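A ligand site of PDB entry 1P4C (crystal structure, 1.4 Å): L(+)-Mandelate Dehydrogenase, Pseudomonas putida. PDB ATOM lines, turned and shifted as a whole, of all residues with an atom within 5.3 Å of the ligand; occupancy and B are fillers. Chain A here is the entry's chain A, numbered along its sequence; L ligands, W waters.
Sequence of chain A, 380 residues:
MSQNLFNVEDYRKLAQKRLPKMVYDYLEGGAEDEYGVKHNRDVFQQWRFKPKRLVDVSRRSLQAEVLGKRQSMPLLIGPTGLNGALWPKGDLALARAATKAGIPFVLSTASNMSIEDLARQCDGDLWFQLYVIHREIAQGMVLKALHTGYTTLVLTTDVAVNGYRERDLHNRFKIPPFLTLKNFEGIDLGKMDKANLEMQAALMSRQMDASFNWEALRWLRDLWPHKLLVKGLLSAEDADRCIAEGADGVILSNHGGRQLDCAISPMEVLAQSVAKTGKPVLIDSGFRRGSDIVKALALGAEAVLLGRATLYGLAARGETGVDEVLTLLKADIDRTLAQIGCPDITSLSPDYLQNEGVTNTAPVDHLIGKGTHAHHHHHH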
ATOM      1  N   TYR A  26      11.429 -12.831 -16.465  1.00  0.00           N
ATOM      2  CA  TYR A  26       9.993 -12.991 -16.615  1.00  0.00           C
ATOM      3  C   TYR A  26       9.278 -12.492 -15.351  1.00  0.00           C
ATOM      4  O   TYR A  26       8.201 -11.907 -15.420  1.00  0.00           O
ATOM      5  CB  TYR A  26       9.669 -14.469 -16.877  1.00  0.00           C
ATOM      6  CG  TYR A  26       8.395 -14.944 -16.251  1.00  0.00           C
ATOM      7  CD1 TYR A  26       7.155 -14.646 -16.808  1.00  0.00           C
ATOM      8  CD2 TYR A  26       8.422 -15.669 -15.057  1.00  0.00           C
ATOM      9  CE1 TYR A  26       5.981 -15.061 -16.203  1.00  0.00           C
ATOM     10  CE2 TYR A  26       7.261 -16.083 -14.448  1.00  0.00           C
ATOM     11  CZ  TYR A  26       6.033 -15.780 -15.023  1.00  0.00           C
ATOM     12  OH  TYR A  26       4.884 -16.200 -14.402  1.00  0.00           O
ATOM     13  N   LEU A  27       9.904 -12.731 -14.200  1.00  0.00           N
ATOM     14  CA  LEU A  27       9.350 -12.324 -12.919  1.00  0.00           C
ATOM     15  C   LEU A  27       9.485 -10.823 -12.640  1.00  0.00           C
ATOM     16  O   LEU A  27       8.521 -10.151 -12.268  1.00  0.00           O
ATOM     17  CB  LEU A  27      10.058 -13.082 -11.784  1.00  0.00           C
ATOM     18  CG  LEU A  27       9.870 -12.545 -10.362  1.00  0.00           C
ATOM     19  CD1 LEU A  27       8.424 -12.674  -9.942  1.00  0.00           C
ATOM     20  CD2 LEU A  27      10.774 -13.306  -9.400  1.00  0.00           C
ATOM     21  N   GLY A  78      -1.262 -11.870  -3.354  1.00  0.00           N
ATOM     22  CA  GLY A  78      -2.068 -11.716  -4.557  1.00  0.00           C
ATOM     23  C   GLY A  78      -1.919 -12.799  -5.591  1.00  0.00           C
ATOM     24  O   GLY A  78      -1.022 -13.632  -5.498  1.00  0.00           O
ATOM     25  N   PRO A  79      -2.783 -12.798  -6.616  1.00  0.00           N
ATOM     26  CA  PRO A  79      -2.729 -13.816  -7.667  1.00  0.00           C
ATOM     27  C   PRO A  79      -1.582 -13.631  -8.652  1.00  0.00           C
ATOM     28  O   PRO A  79      -1.440 -12.572  -9.252  1.00  0.00           O
ATOM     29  CB  PRO A  79      -4.096 -13.667  -8.343  1.00  0.00           C
ATOM     30  CG  PRO A  79      -4.356 -12.188  -8.227  1.00  0.00           C
ATOM     31  CD  PRO A  79      -3.914 -11.880  -6.809  1.00  0.00           C
ATOM     32  N   THR A  80      -0.763 -14.670  -8.789  1.00  0.00           N
ATOM     33  CA  THR A  80       0.337 -14.635  -9.738  1.00  0.00           C
ATOM     34  C   THR A  80       0.369 -15.992 -10.418  1.00  0.00           C
ATOM     35  O   THR A  80       0.313 -17.033  -9.760  1.00  0.00           O
ATOM     36  CB  THR A  80       1.701 -14.349  -9.046  1.00  0.00           C
ATOM     37  OG1 THR A  80       1.930 -15.307  -8.004  1.00  0.00           O
ATOM     38  CG2 THR A  80       1.698 -12.944  -8.449  1.00  0.00           C
ATOM     39  N   GLY A  81       0.414 -15.978 -11.745  1.00  0.00           N
ATOM     40  CA  GLY A  81       0.407 -17.229 -12.488  1.00  0.00           C
ATOM     41  C   GLY A  81       1.780 -17.880 -12.621  1.00  0.00           C
ATOM     42  O   GLY A  81       2.815 -17.239 -12.439  1.00  0.00           O
ATOM     43  N   SER A 108      -4.330 -17.980  -8.876  1.00  0.00           N
ATOM     44  CA  SER A 108      -4.459 -17.477 -10.242  1.00  0.00           C
ATOM     45  C   SER A 108      -5.142 -18.477 -11.160  1.00  0.00           C
ATOM     46  O   SER A 108      -5.052 -19.689 -10.959  1.00  0.00           O
ATOM     47  CB  SER A 108      -3.084 -17.157 -10.810  1.00  0.00           C
ATOM     48  OG  SER A 108      -3.136 -16.960 -12.212  1.00  0.00           O
ATOM     49  N   THR A 109      -5.827 -17.972 -12.175  1.00  0.00           N
ATOM     50  CA  THR A 109      -6.472 -18.846 -13.149  1.00  0.00           C
ATOM     51  C   THR A 109      -5.352 -19.597 -13.876  1.00  0.00           C
ATOM     52  O   THR A 109      -5.548 -20.723 -14.339  1.00  0.00           O
ATOM     53  CB  THR A 109      -7.285 -18.040 -14.180  1.00  0.00           C
ATOM     54  OG1 THR A 109      -8.523 -17.632 -13.598  1.00  0.00           O
ATOM     55  CG2 THR A 109      -7.560 -18.871 -15.424  1.00  0.00           C
ATOM     56  N   ALA A 110      -4.183 -18.972 -13.953  1.00  0.00           N
ATOM     57  CA  ALA A 110      -3.017 -19.567 -14.615  1.00  0.00           C
ATOM     58  C   ALA A 110      -2.079 -20.250 -13.629  1.00  0.00           C
ATOM     59  O   ALA A 110      -0.860 -20.298 -13.843  1.00  0.00           O
ATOM     60  CB  ALA A 110      -2.259 -18.492 -15.392  1.00  0.00           C
ATOM     61  N   GLN A 129      -8.792 -15.965  -8.388  1.00  0.00           N
ATOM     62  CA  GLN A 129      -8.691 -14.888  -9.366  1.00  0.00           C
ATOM     63  C   GLN A 129      -9.056 -15.457 -10.728  1.00  0.00           C
ATOM     64  O   GLN A 129      -8.458 -16.435 -11.187  1.00  0.00           O
ATOM     65  CB  GLN A 129      -7.281 -14.318  -9.404  1.00  0.00           C
ATOM     66  CG  GLN A 129      -7.053 -13.298 -10.535  1.00  0.00           C
ATOM     67  CD  GLN A 129      -6.585 -13.928 -11.838  1.00  0.00           C
ATOM     68  OE1 GLN A 129      -7.081 -13.612 -12.917  1.00  0.00           O
ATOM     69  NE2 GLN A 129      -5.608 -14.810 -11.733  1.00  0.00           N
ATOM     70  N   TYR A 131      -9.657 -15.179 -14.897  1.00  0.00           N
ATOM     71  CA  TYR A 131      -9.310 -14.598 -16.189  1.00  0.00           C
ATOM     72  C   TYR A 131     -10.348 -15.244 -17.086  1.00  0.00           C
ATOM     73  O   TYR A 131     -10.562 -16.450 -17.006  1.00  0.00           O
ATOM     74  CB  TYR A 131      -7.931 -15.048 -16.665  1.00  0.00           C
ATOM     75  CG  TYR A 131      -6.769 -14.197 -16.214  1.00  0.00           C
ATOM     76  CD1 TYR A 131      -6.855 -12.811 -16.202  1.00  0.00           C
ATOM     77  CD2 TYR A 131      -5.567 -14.792 -15.863  1.00  0.00           C
ATOM     78  CE1 TYR A 131      -5.751 -12.027 -15.871  1.00  0.00           C
ATOM     79  CE2 TYR A 131      -4.462 -14.025 -15.531  1.00  0.00           C
ATOM     80  CZ  TYR A 131      -4.557 -12.646 -15.538  1.00  0.00           C
ATOM     81  OH  TYR A 131      -3.456 -11.897 -15.218  1.00  0.00           O
ATOM     82  N   THR A 156      -9.861 -10.249 -12.805  1.00  0.00           N
ATOM     83  CA  THR A 156      -8.775  -9.395 -13.277  1.00  0.00           C
ATOM     84  C   THR A 156      -9.156  -8.895 -14.660  1.00  0.00           C
ATOM     85  O   THR A 156      -9.412  -9.672 -15.568  1.00  0.00           O
ATOM     86  CB  THR A 156      -7.445 -10.152 -13.319  1.00  0.00           C
ATOM     87  OG1 THR A 156      -7.125 -10.581 -11.992  1.00  0.00           O
ATOM     88  CG2 THR A 156      -6.330  -9.246 -13.824  1.00  0.00           C
ATOM     89  N   LYS A 231     -10.383  -6.423 -10.102  1.00  0.00           N
ATOM     90  CA  LYS A 231      -8.972  -6.055 -10.055  1.00  0.00           C
ATOM     91  C   LYS A 231      -8.452  -5.439 -11.341  1.00  0.00           C
ATOM     92  O   LYS A 231      -8.879  -5.822 -12.437  1.00  0.00           O
ATOM     93  CB  LYS A 231      -8.165  -7.311  -9.701  1.00  0.00           C
ATOM     94  CG  LYS A 231      -6.642  -7.162  -9.696  1.00  0.00           C
ATOM     95  CD  LYS A 231      -6.018  -8.428  -9.113  1.00  0.00           C
ATOM     96  CE  LYS A 231      -4.491  -8.387  -9.081  1.00  0.00           C
ATOM     97  NZ  LYS A 231      -3.883  -8.645 -10.421  1.00  0.00           N
ATOM     98  N   SER A 253      -4.948  -1.386  -9.323  1.00  0.00           N
ATOM     99  CA  SER A 253      -3.718  -2.044  -9.704  1.00  0.00           C
ATOM    100  C   SER A 253      -3.309  -1.776 -11.138  1.00  0.00           C
ATOM    101  O   SER A 253      -4.174  -1.562 -11.987  1.00  0.00           O
ATOM    102  CB  SER A 253      -3.921  -3.563  -9.534  1.00  0.00           C
ATOM    103  OG  SER A 253      -2.884  -4.331 -10.123  1.00  0.00           O
ATOM    104  N   HIS A 255      -1.140  -3.998 -12.428  1.00  0.00           N
ATOM    105  CA  HIS A 255      -0.561  -5.313 -12.685  1.00  0.00           C
ATOM    106  C   HIS A 255       0.955  -5.289 -12.532  1.00  0.00           C
ATOM    107  O   HIS A 255       1.677  -5.922 -13.307  1.00  0.00           O
ATOM    108  CB  HIS A 255      -0.946  -5.752 -14.101  1.00  0.00           C
ATOM    109  CG  HIS A 255      -1.067  -7.230 -14.275  1.00  0.00           C
ATOM    110  ND1 HIS A 255      -2.290  -7.855 -14.397  1.00  0.00           N
ATOM    111  CD2 HIS A 255      -0.129  -8.194 -14.382  1.00  0.00           C
ATOM    112  CE1 HIS A 255      -2.089  -9.154 -14.568  1.00  0.00           C
ATOM    113  NE2 HIS A 255      -0.792  -9.383 -14.563  1.00  0.00           N
ATOM    114  N   GLY A 256       1.442  -4.563 -11.524  1.00  0.00           N
ATOM    115  CA  GLY A 256       2.870  -4.496 -11.279  1.00  0.00           C
ATOM    116  C   GLY A 256       3.709  -3.960 -12.429  1.00  0.00           C
ATOM    117  O   GLY A 256       4.843  -4.385 -12.619  1.00  0.00           O
ATOM    118  N   ARG A 258       3.408  -4.501 -15.495  1.00  0.00           N
ATOM    119  CA  ARG A 258       3.625  -5.523 -16.521  1.00  0.00           C
ATOM    120  C   ARG A 258       2.741  -5.419 -17.752  1.00  0.00           C
ATOM    121  O   ARG A 258       2.958  -6.155 -18.723  1.00  0.00           O
ATOM    122  CB  ARG A 258       3.439  -6.906 -15.889  1.00  0.00           C
ATOM    123  CG  ARG A 258       4.452  -7.210 -14.793  1.00  0.00           C
ATOM    124  CD  ARG A 258       4.039  -8.409 -13.963  1.00  0.00           C
ATOM    125  NE  ARG A 258       4.126  -9.696 -14.668  1.00  0.00           N
ATOM    126  CZ  ARG A 258       5.261 -10.333 -14.925  1.00  0.00           C
ATOM    127  NH1 ARG A 258       6.429  -9.827 -14.541  1.00  0.00           N
ATOM    128  NH2 ARG A 258       5.228 -11.524 -15.512  1.00  0.00           N
ATOM    129  N   ASP A 284      -2.544  -2.894  -5.021  1.00  0.00           N
ATOM    130  CA  ASP A 284      -1.256  -3.567  -5.190  1.00  0.00           C
ATOM    131  C   ASP A 284      -0.467  -2.748  -6.213  1.00  0.00           C
ATOM    132  O   ASP A 284      -0.925  -1.694  -6.649  1.00  0.00           O
ATOM    133  CB  ASP A 284      -1.409  -5.043  -5.641  1.00  0.00           C
ATOM    134  CG  ASP A 284      -1.883  -5.215  -7.074  1.00  0.00           C
ATOM    135  OD1 ASP A 284      -1.723  -4.295  -7.896  1.00  0.00           O
ATOM    136  OD2 ASP A 284      -2.407  -6.303  -7.399  1.00  0.00           O
ATOM    137  N   SER A 285       0.735  -3.235  -6.526  1.00  0.00           N
ATOM    138  CA  SER A 285       1.651  -2.640  -7.494  1.00  0.00           C
ATOM    139  C   SER A 285       2.704  -1.722  -6.903  1.00  0.00           C
ATOM    140  O   SER A 285       2.444  -0.545  -6.608  1.00  0.00           O
ATOM    141  CB  SER A 285       0.894  -1.889  -8.610  1.00  0.00           C
ATOM    142  OG  SER A 285       0.049  -2.768  -9.342  1.00  0.00           O
ATOM    143  N   GLY A 286       3.903  -2.268  -6.730  1.00  0.00           N
ATOM    144  CA  GLY A 286       5.020  -1.502  -6.211  1.00  0.00           C
ATOM    145  C   GLY A 286       5.345  -1.629  -4.743  1.00  0.00           C
ATOM    146  O   GLY A 286       6.342  -1.073  -4.283  1.00  0.00           O
ATOM    147  N   PHE A 287       4.537  -2.365  -3.975  1.00  0.00           N
ATOM    148  CA  PHE A 287       4.773  -2.467  -2.538  1.00  0.00           C
ATOM    149  C   PHE A 287       5.958  -3.357  -2.178  1.00  0.00           C
ATOM    150  O   PHE A 287       6.006  -4.528  -2.560  1.00  0.00           O
ATOM    151  CB  PHE A 287       3.504  -2.943  -1.825  1.00  0.00           C
ATOM    152  CG  PHE A 287       2.377  -1.974  -1.935  1.00  0.00           C
ATOM    153  CD1 PHE A 287       1.563  -1.943  -3.063  1.00  0.00           C
ATOM    154  CD2 PHE A 287       2.153  -1.028  -0.925  1.00  0.00           C
ATOM    155  CE1 PHE A 287       0.560  -0.982  -3.195  1.00  0.00           C
ATOM    156  CE2 PHE A 287       1.159  -0.073  -1.059  1.00  0.00           C
ATOM    157  CZ  PHE A 287       0.361  -0.053  -2.190  1.00  0.00           C
ATOM    158  N   ARG A 288       6.914  -2.798  -1.445  1.00  0.00           N
ATOM    159  CA  ARG A 288       8.110  -3.523  -1.047  1.00  0.00           C
ATOM    160  C   ARG A 288       8.502  -3.336   0.413  1.00  0.00           C
ATOM    161  O   ARG A 288       9.056  -4.249   1.027  1.00  0.00           O
ATOM    162  CB  ARG A 288       9.294  -3.105  -1.917  1.00  0.00           C
ATOM    163  CG  ARG A 288       9.104  -3.311  -3.412  1.00  0.00           C
ATOM    164  CD  ARG A 288       9.124  -4.780  -3.826  1.00  0.00           C
ATOM    165  NE  ARG A 288       9.038  -4.899  -5.287  1.00  0.00           N
ATOM    166  CZ  ARG A 288       7.894  -4.819  -5.963  1.00  0.00           C
ATOM    167  NH1 ARG A 288       6.743  -4.636  -5.337  1.00  0.00           N
ATOM    168  NH2 ARG A 288       7.923  -4.881  -7.295  1.00  0.00           N
ATOM    169  N   LEU A 305      -2.205  -6.077  -1.527  1.00  0.00           N
ATOM    170  CA  LEU A 305      -1.868  -7.396  -2.045  1.00  0.00           C
ATOM    171  C   LEU A 305      -0.420  -7.385  -2.480  1.00  0.00           C
ATOM    172  O   LEU A 305       0.041  -6.440  -3.123  1.00  0.00           O
ATOM    173  CB  LEU A 305      -2.740  -7.787  -3.233  1.00  0.00           C
ATOM    174  CG  LEU A 305      -4.222  -8.034  -2.949  1.00  0.00           C
ATOM    175  CD1 LEU A 305      -4.978  -6.715  -3.028  1.00  0.00           C
ATOM    176  CD2 LEU A 305      -4.796  -9.007  -3.970  1.00  0.00           C
ATOM    177  N   LEU A 306       0.299  -8.434  -2.110  1.00  0.00           N
ATOM    178  CA  LEU A 306       1.697  -8.570  -2.472  1.00  0.00           C
ATOM    179  C   LEU A 306       1.819  -9.407  -3.741  1.00  0.00           C
ATOM    180  O   LEU A 306       1.134 -10.422  -3.899  1.00  0.00           O
ATOM    181  CB  LEU A 306       2.477  -9.256  -1.345  1.00  0.00           C
ATOM    182  CG  LEU A 306       2.440  -8.551   0.006  1.00  0.00           C
ATOM    183  CD1 LEU A 306       3.194  -9.384   1.018  1.00  0.00           C
ATOM    184  CD2 LEU A 306       3.048  -7.155  -0.118  1.00  0.00           C
ATOM    185  N   GLY A 307       2.685  -8.960  -4.636  1.00  0.00           N
ATOM    186  CA  GLY A 307       2.922  -9.681  -5.861  1.00  0.00           C
ATOM    187  C   GLY A 307       4.353 -10.192  -5.813  1.00  0.00           C
ATOM    188  O   GLY A 307       4.637 -11.238  -5.233  1.00  0.00           O
ATOM    189  N   ARG A 308       5.268  -9.431  -6.390  1.00  0.00           N
ATOM    190  CA  ARG A 308       6.667  -9.848  -6.399  1.00  0.00           C
ATOM    191  C   ARG A 308       7.333 -10.021  -5.035  1.00  0.00           C
ATOM    192  O   ARG A 308       8.188 -10.876  -4.894  1.00  0.00           O
ATOM    193  CB  ARG A 308       7.502  -8.890  -7.246  1.00  0.00           C
ATOM    194  CG  ARG A 308       7.188  -8.903  -8.729  1.00  0.00           C
ATOM    195  CD  ARG A 308       8.165  -7.991  -9.448  1.00  0.00           C
ATOM    196  NE  ARG A 308       7.878  -7.756 -10.860  1.00  0.00           N
ATOM    197  CZ  ARG A 308       7.022  -6.843 -11.318  1.00  0.00           C
ATOM    198  NH1 ARG A 308       6.340  -6.084 -10.473  1.00  0.00           N
ATOM    199  NH2 ARG A 308       6.900  -6.649 -12.629  1.00  0.00           N
ATOM    200  N   ALA A 309       6.960  -9.214  -4.044  1.00  0.00           N
ATOM    201  CA  ALA A 309       7.615  -9.316  -2.734  1.00  0.00           C
ATOM    202  C   ALA A 309       7.661 -10.730  -2.187  1.00  0.00           C
ATOM    203  O   ALA A 309       8.733 -11.217  -1.810  1.00  0.00           O
ATOM    204  CB  ALA A 309       6.936  -8.385  -1.726  1.00  0.00           C
ATOM    205  N   LEU A 311       6.981 -13.420  -3.940  1.00  0.00           N
ATOM    206  CA  LEU A 311       7.521 -14.315  -4.959  1.00  0.00           C
ATOM    207  C   LEU A 311       9.056 -14.362  -4.835  1.00  0.00           C
ATOM    208  O   LEU A 311       9.671 -15.363  -5.194  1.00  0.00           O
ATOM    209  CB  LEU A 311       7.128 -13.858  -6.372  1.00  0.00           C
ATOM    210  CG  LEU A 311       5.654 -14.030  -6.723  1.00  0.00           C
ATOM    211  CD1 LEU A 311       5.436 -13.680  -8.188  1.00  0.00           C
ATOM    212  CD2 LEU A 311       5.206 -15.471  -6.453  1.00  0.00           C
HETATM  213  N1  LIG L   1      -2.403 -10.897 -11.719  1.00  0.00           N
HETATM  214  C1  LIG L   1      -3.556 -11.631 -11.858  1.00  0.00           C
HETATM  215  O1  LIG L   1      -4.602 -11.215 -11.566  1.00  0.00           O
HETATM  216  N2  LIG L   1      -3.409 -13.002 -12.347  1.00  0.00           N
HETATM  217  C2  LIG L   1      -2.191 -13.637 -12.742  1.00  0.00           C
HETATM  218  O2  LIG L   1      -2.115 -14.797 -13.146  1.00  0.00           O
HETATM  219  C3  LIG L   1      -0.955 -12.812 -12.571  1.00  0.00           C
HETATM  220  N3  LIG L   1       0.280 -13.306 -12.818  1.00  0.00           N
HETATM  221  C4  LIG L   1       1.435 -12.595 -12.473  1.00  0.00           C
HETATM  222  C5  LIG L   1       2.732 -13.213 -12.604  1.00  0.00           C
HETATM  223  C6  LIG L   1       3.965 -12.568 -12.136  1.00  0.00           C
HETATM  224  C7  LIG L   1       5.260 -13.296 -12.266  1.00  0.00           C
HETATM  225  C8  LIG L   1       3.865 -11.170 -11.507  1.00  0.00           C
HETATM  226  C9  LIG L   1       5.026 -10.411 -10.933  1.00  0.00           C
HETATM  227  C10 LIG L   1       2.583 -10.571 -11.422  1.00  0.00           C
HETATM  228  C11 LIG L   1       1.340 -11.204 -11.860  1.00  0.00           C
HETATM  229  N4  LIG L   1      -0.023 -10.685 -11.714  1.00  0.00           N
HETATM  230  C12 LIG L   1      -1.204 -11.412 -12.014  1.00  0.00           C
HETATM  231  C13 LIG L   1      -0.175  -9.332 -11.128  1.00  0.00           C
HETATM  232  C14 LIG L   1      -0.232  -9.370  -9.599  1.00  0.00           C
HETATM  233  O3  LIG L   1      -1.441  -9.841  -9.150  1.00  0.00           O
HETATM  234  C15 LIG L   1      -0.035  -8.003  -8.977  1.00  0.00           C
HETATM  235  O4  LIG L   1      -0.949  -7.046  -9.628  1.00  0.00           O
HETATM  236  C16 LIG L   1       1.340  -7.372  -9.156  1.00  0.00           C
HETATM  237  O5  LIG L   1       2.394  -8.301  -9.002  1.00  0.00           O
HETATM  238  C17 LIG L   1       1.488  -6.286  -8.132  1.00  0.00           C
HETATM  239  O6  LIG L   1       2.779  -5.611  -8.205  1.00  0.00           O
HETATM  240  P1  LIG L   1       4.115  -5.933  -7.518  1.00  0.00           P
HETATM  241  O7  LIG L   1       5.002  -4.722  -7.584  1.00  0.00           O
HETATM  242  O8  LIG L   1       4.667  -7.130  -8.243  1.00  0.00           O
HETATM  243  O9  LIG L   1       3.722  -6.260  -6.106  1.00  0.00           O
HETATM  244  O   HOH W   1      -2.182  -8.990  -6.435  1.00  0.00           O
HETATM  245  O   HOH W   2       2.014  -4.926  -4.626  1.00  0.00           O
HETATM  246  O   HOH W   3       5.342  -2.913  -9.683  1.00  0.00           O
HETATM  247  O   HOH W   4      -0.336 -15.450 -15.199  1.00  0.00           O
HETATM  248  O   HOH W   5       4.480 -16.149 -10.588  1.00  0.00           O
HETATM  249  O   HOH W   6       4.949  -7.065  -3.841  1.00  0.00           O
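Water W2 lies within hydrogen-bond range of an oxygen (O9) of the ligand (2.6 Å), the backbone NH (N) of Ser 285 (2.8 Å) and the backbone carbonyl oxygen (O) of Leu 305 (2.9 Å).
Water W3 lies within hydrogen-bond range of an oxygen (O7) of the ligand (2.8 Å), the backbone carbonyl oxygen of Gly 256 (3.3 Å), the backbone NH of Gly 286 (3.3 Å) and the guanidinium group of Arg 308 (3.4 Å).
Water W1 lies within hydrogen-bond range of OD2 of Asp 284 (2.9 Å) and O3 of the ligand (2.9 Å).
A nitrogen (N2) of the ligand is in hydrogen-bond range of the side-chain hydroxyl of Tyr 131, 3.1 Å away.
An oxygen (O2) of the ligand is in hydrogen-bond range of the side-chain hydroxyl (OG) of Ser 108, 2.6 Å away.
The backbone NH (N) of Arg 308 is in hydrogen-bond range of an oxygen (O8) of the ligand (3.0 Å).
The side-chain hydroxyl (OG) of Ser 253 is in hydrogen-bond range of an oxygen (O4) of the ligand, at 3.4 Å.
The backbone NH (N) of Gly 307 is in hydrogen-bond range of an oxygen (O9) of the ligand, 3.2 Å away.
The backbone NH (N) of Gly 286 lies within hydrogen-bond range of an oxygen (O7) of the ligand (2.8 Å).
OD2 of Asp 284 is in hydrogen-bond range of O4 of the ligand (2.8 Å).
NH1 of Arg 288 lies within salt-bridge range of O7 of the ligand.
O of Pro 79 is in hydrogen-bond range of O3 of the ligand (2.7 Å).
The guanidinium group (NH1) of Arg 308 is in salt-bridge range of an oxygen (O8) of the ligand, at 3.0 Å.
The backbone NH (N) of Gly 81 is in hydrogen-bond range of a nitrogen (N3) of the ligand.
The side-chain amide nitrogen (NE2) of Gln 129 sits close to a nitrogen (N2) of the ligand, at 2.9 Å.
O1 of the ligand is in hydrogen-bond range of OG1 of Thr 156, at 2.6 Å.
The side-chain amino group (NZ) of Lys 231 is in hydrogen-bond range of an oxygen (O1) of the ligand (2.9 Å).
OE1 of Gln 129 lies close to OG1 of Thr 156.
The backbone carbonyl oxygen of Tyr 26 is in hydrogen-bond range of the guanidinium group of Arg 258, 2.9 Å away.
OD1 of Asp 284 lies within hydrogen-bond range of OG of Ser 285, 2.8 Å away.
NE2 of Gln 129 sits close to OG of Ser 108 (3.3 Å).
The guanidinium group of Arg 258 is in hydrogen-bond range of the backbone carbonyl oxygen of Leu 27, at 3.1 Å.
NE of Arg 308 sits at hydrogen-bond distance from O of Leu 27.
The backbone NH (N) of Tyr 131 is in hydrogen-bond range of the side-chain hydroxyl (OG1) of Thr 109, 3.0 Å away.
N of His 255 lies within hydrogen-bond range of OG of Ser 253, at 2.9 Å.
N4 of the ligand lies close to NE2 of His 255 (3.2 Å).
Residues that only touch the ligand: Tyr 26 (3.6 Å), Leu 27 (3.8 Å), Thr 80 (3.4 Å), Gly 256 (3.3 Å), Arg 258 (3.5 Å) and Ser 285 (3.3 Å).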
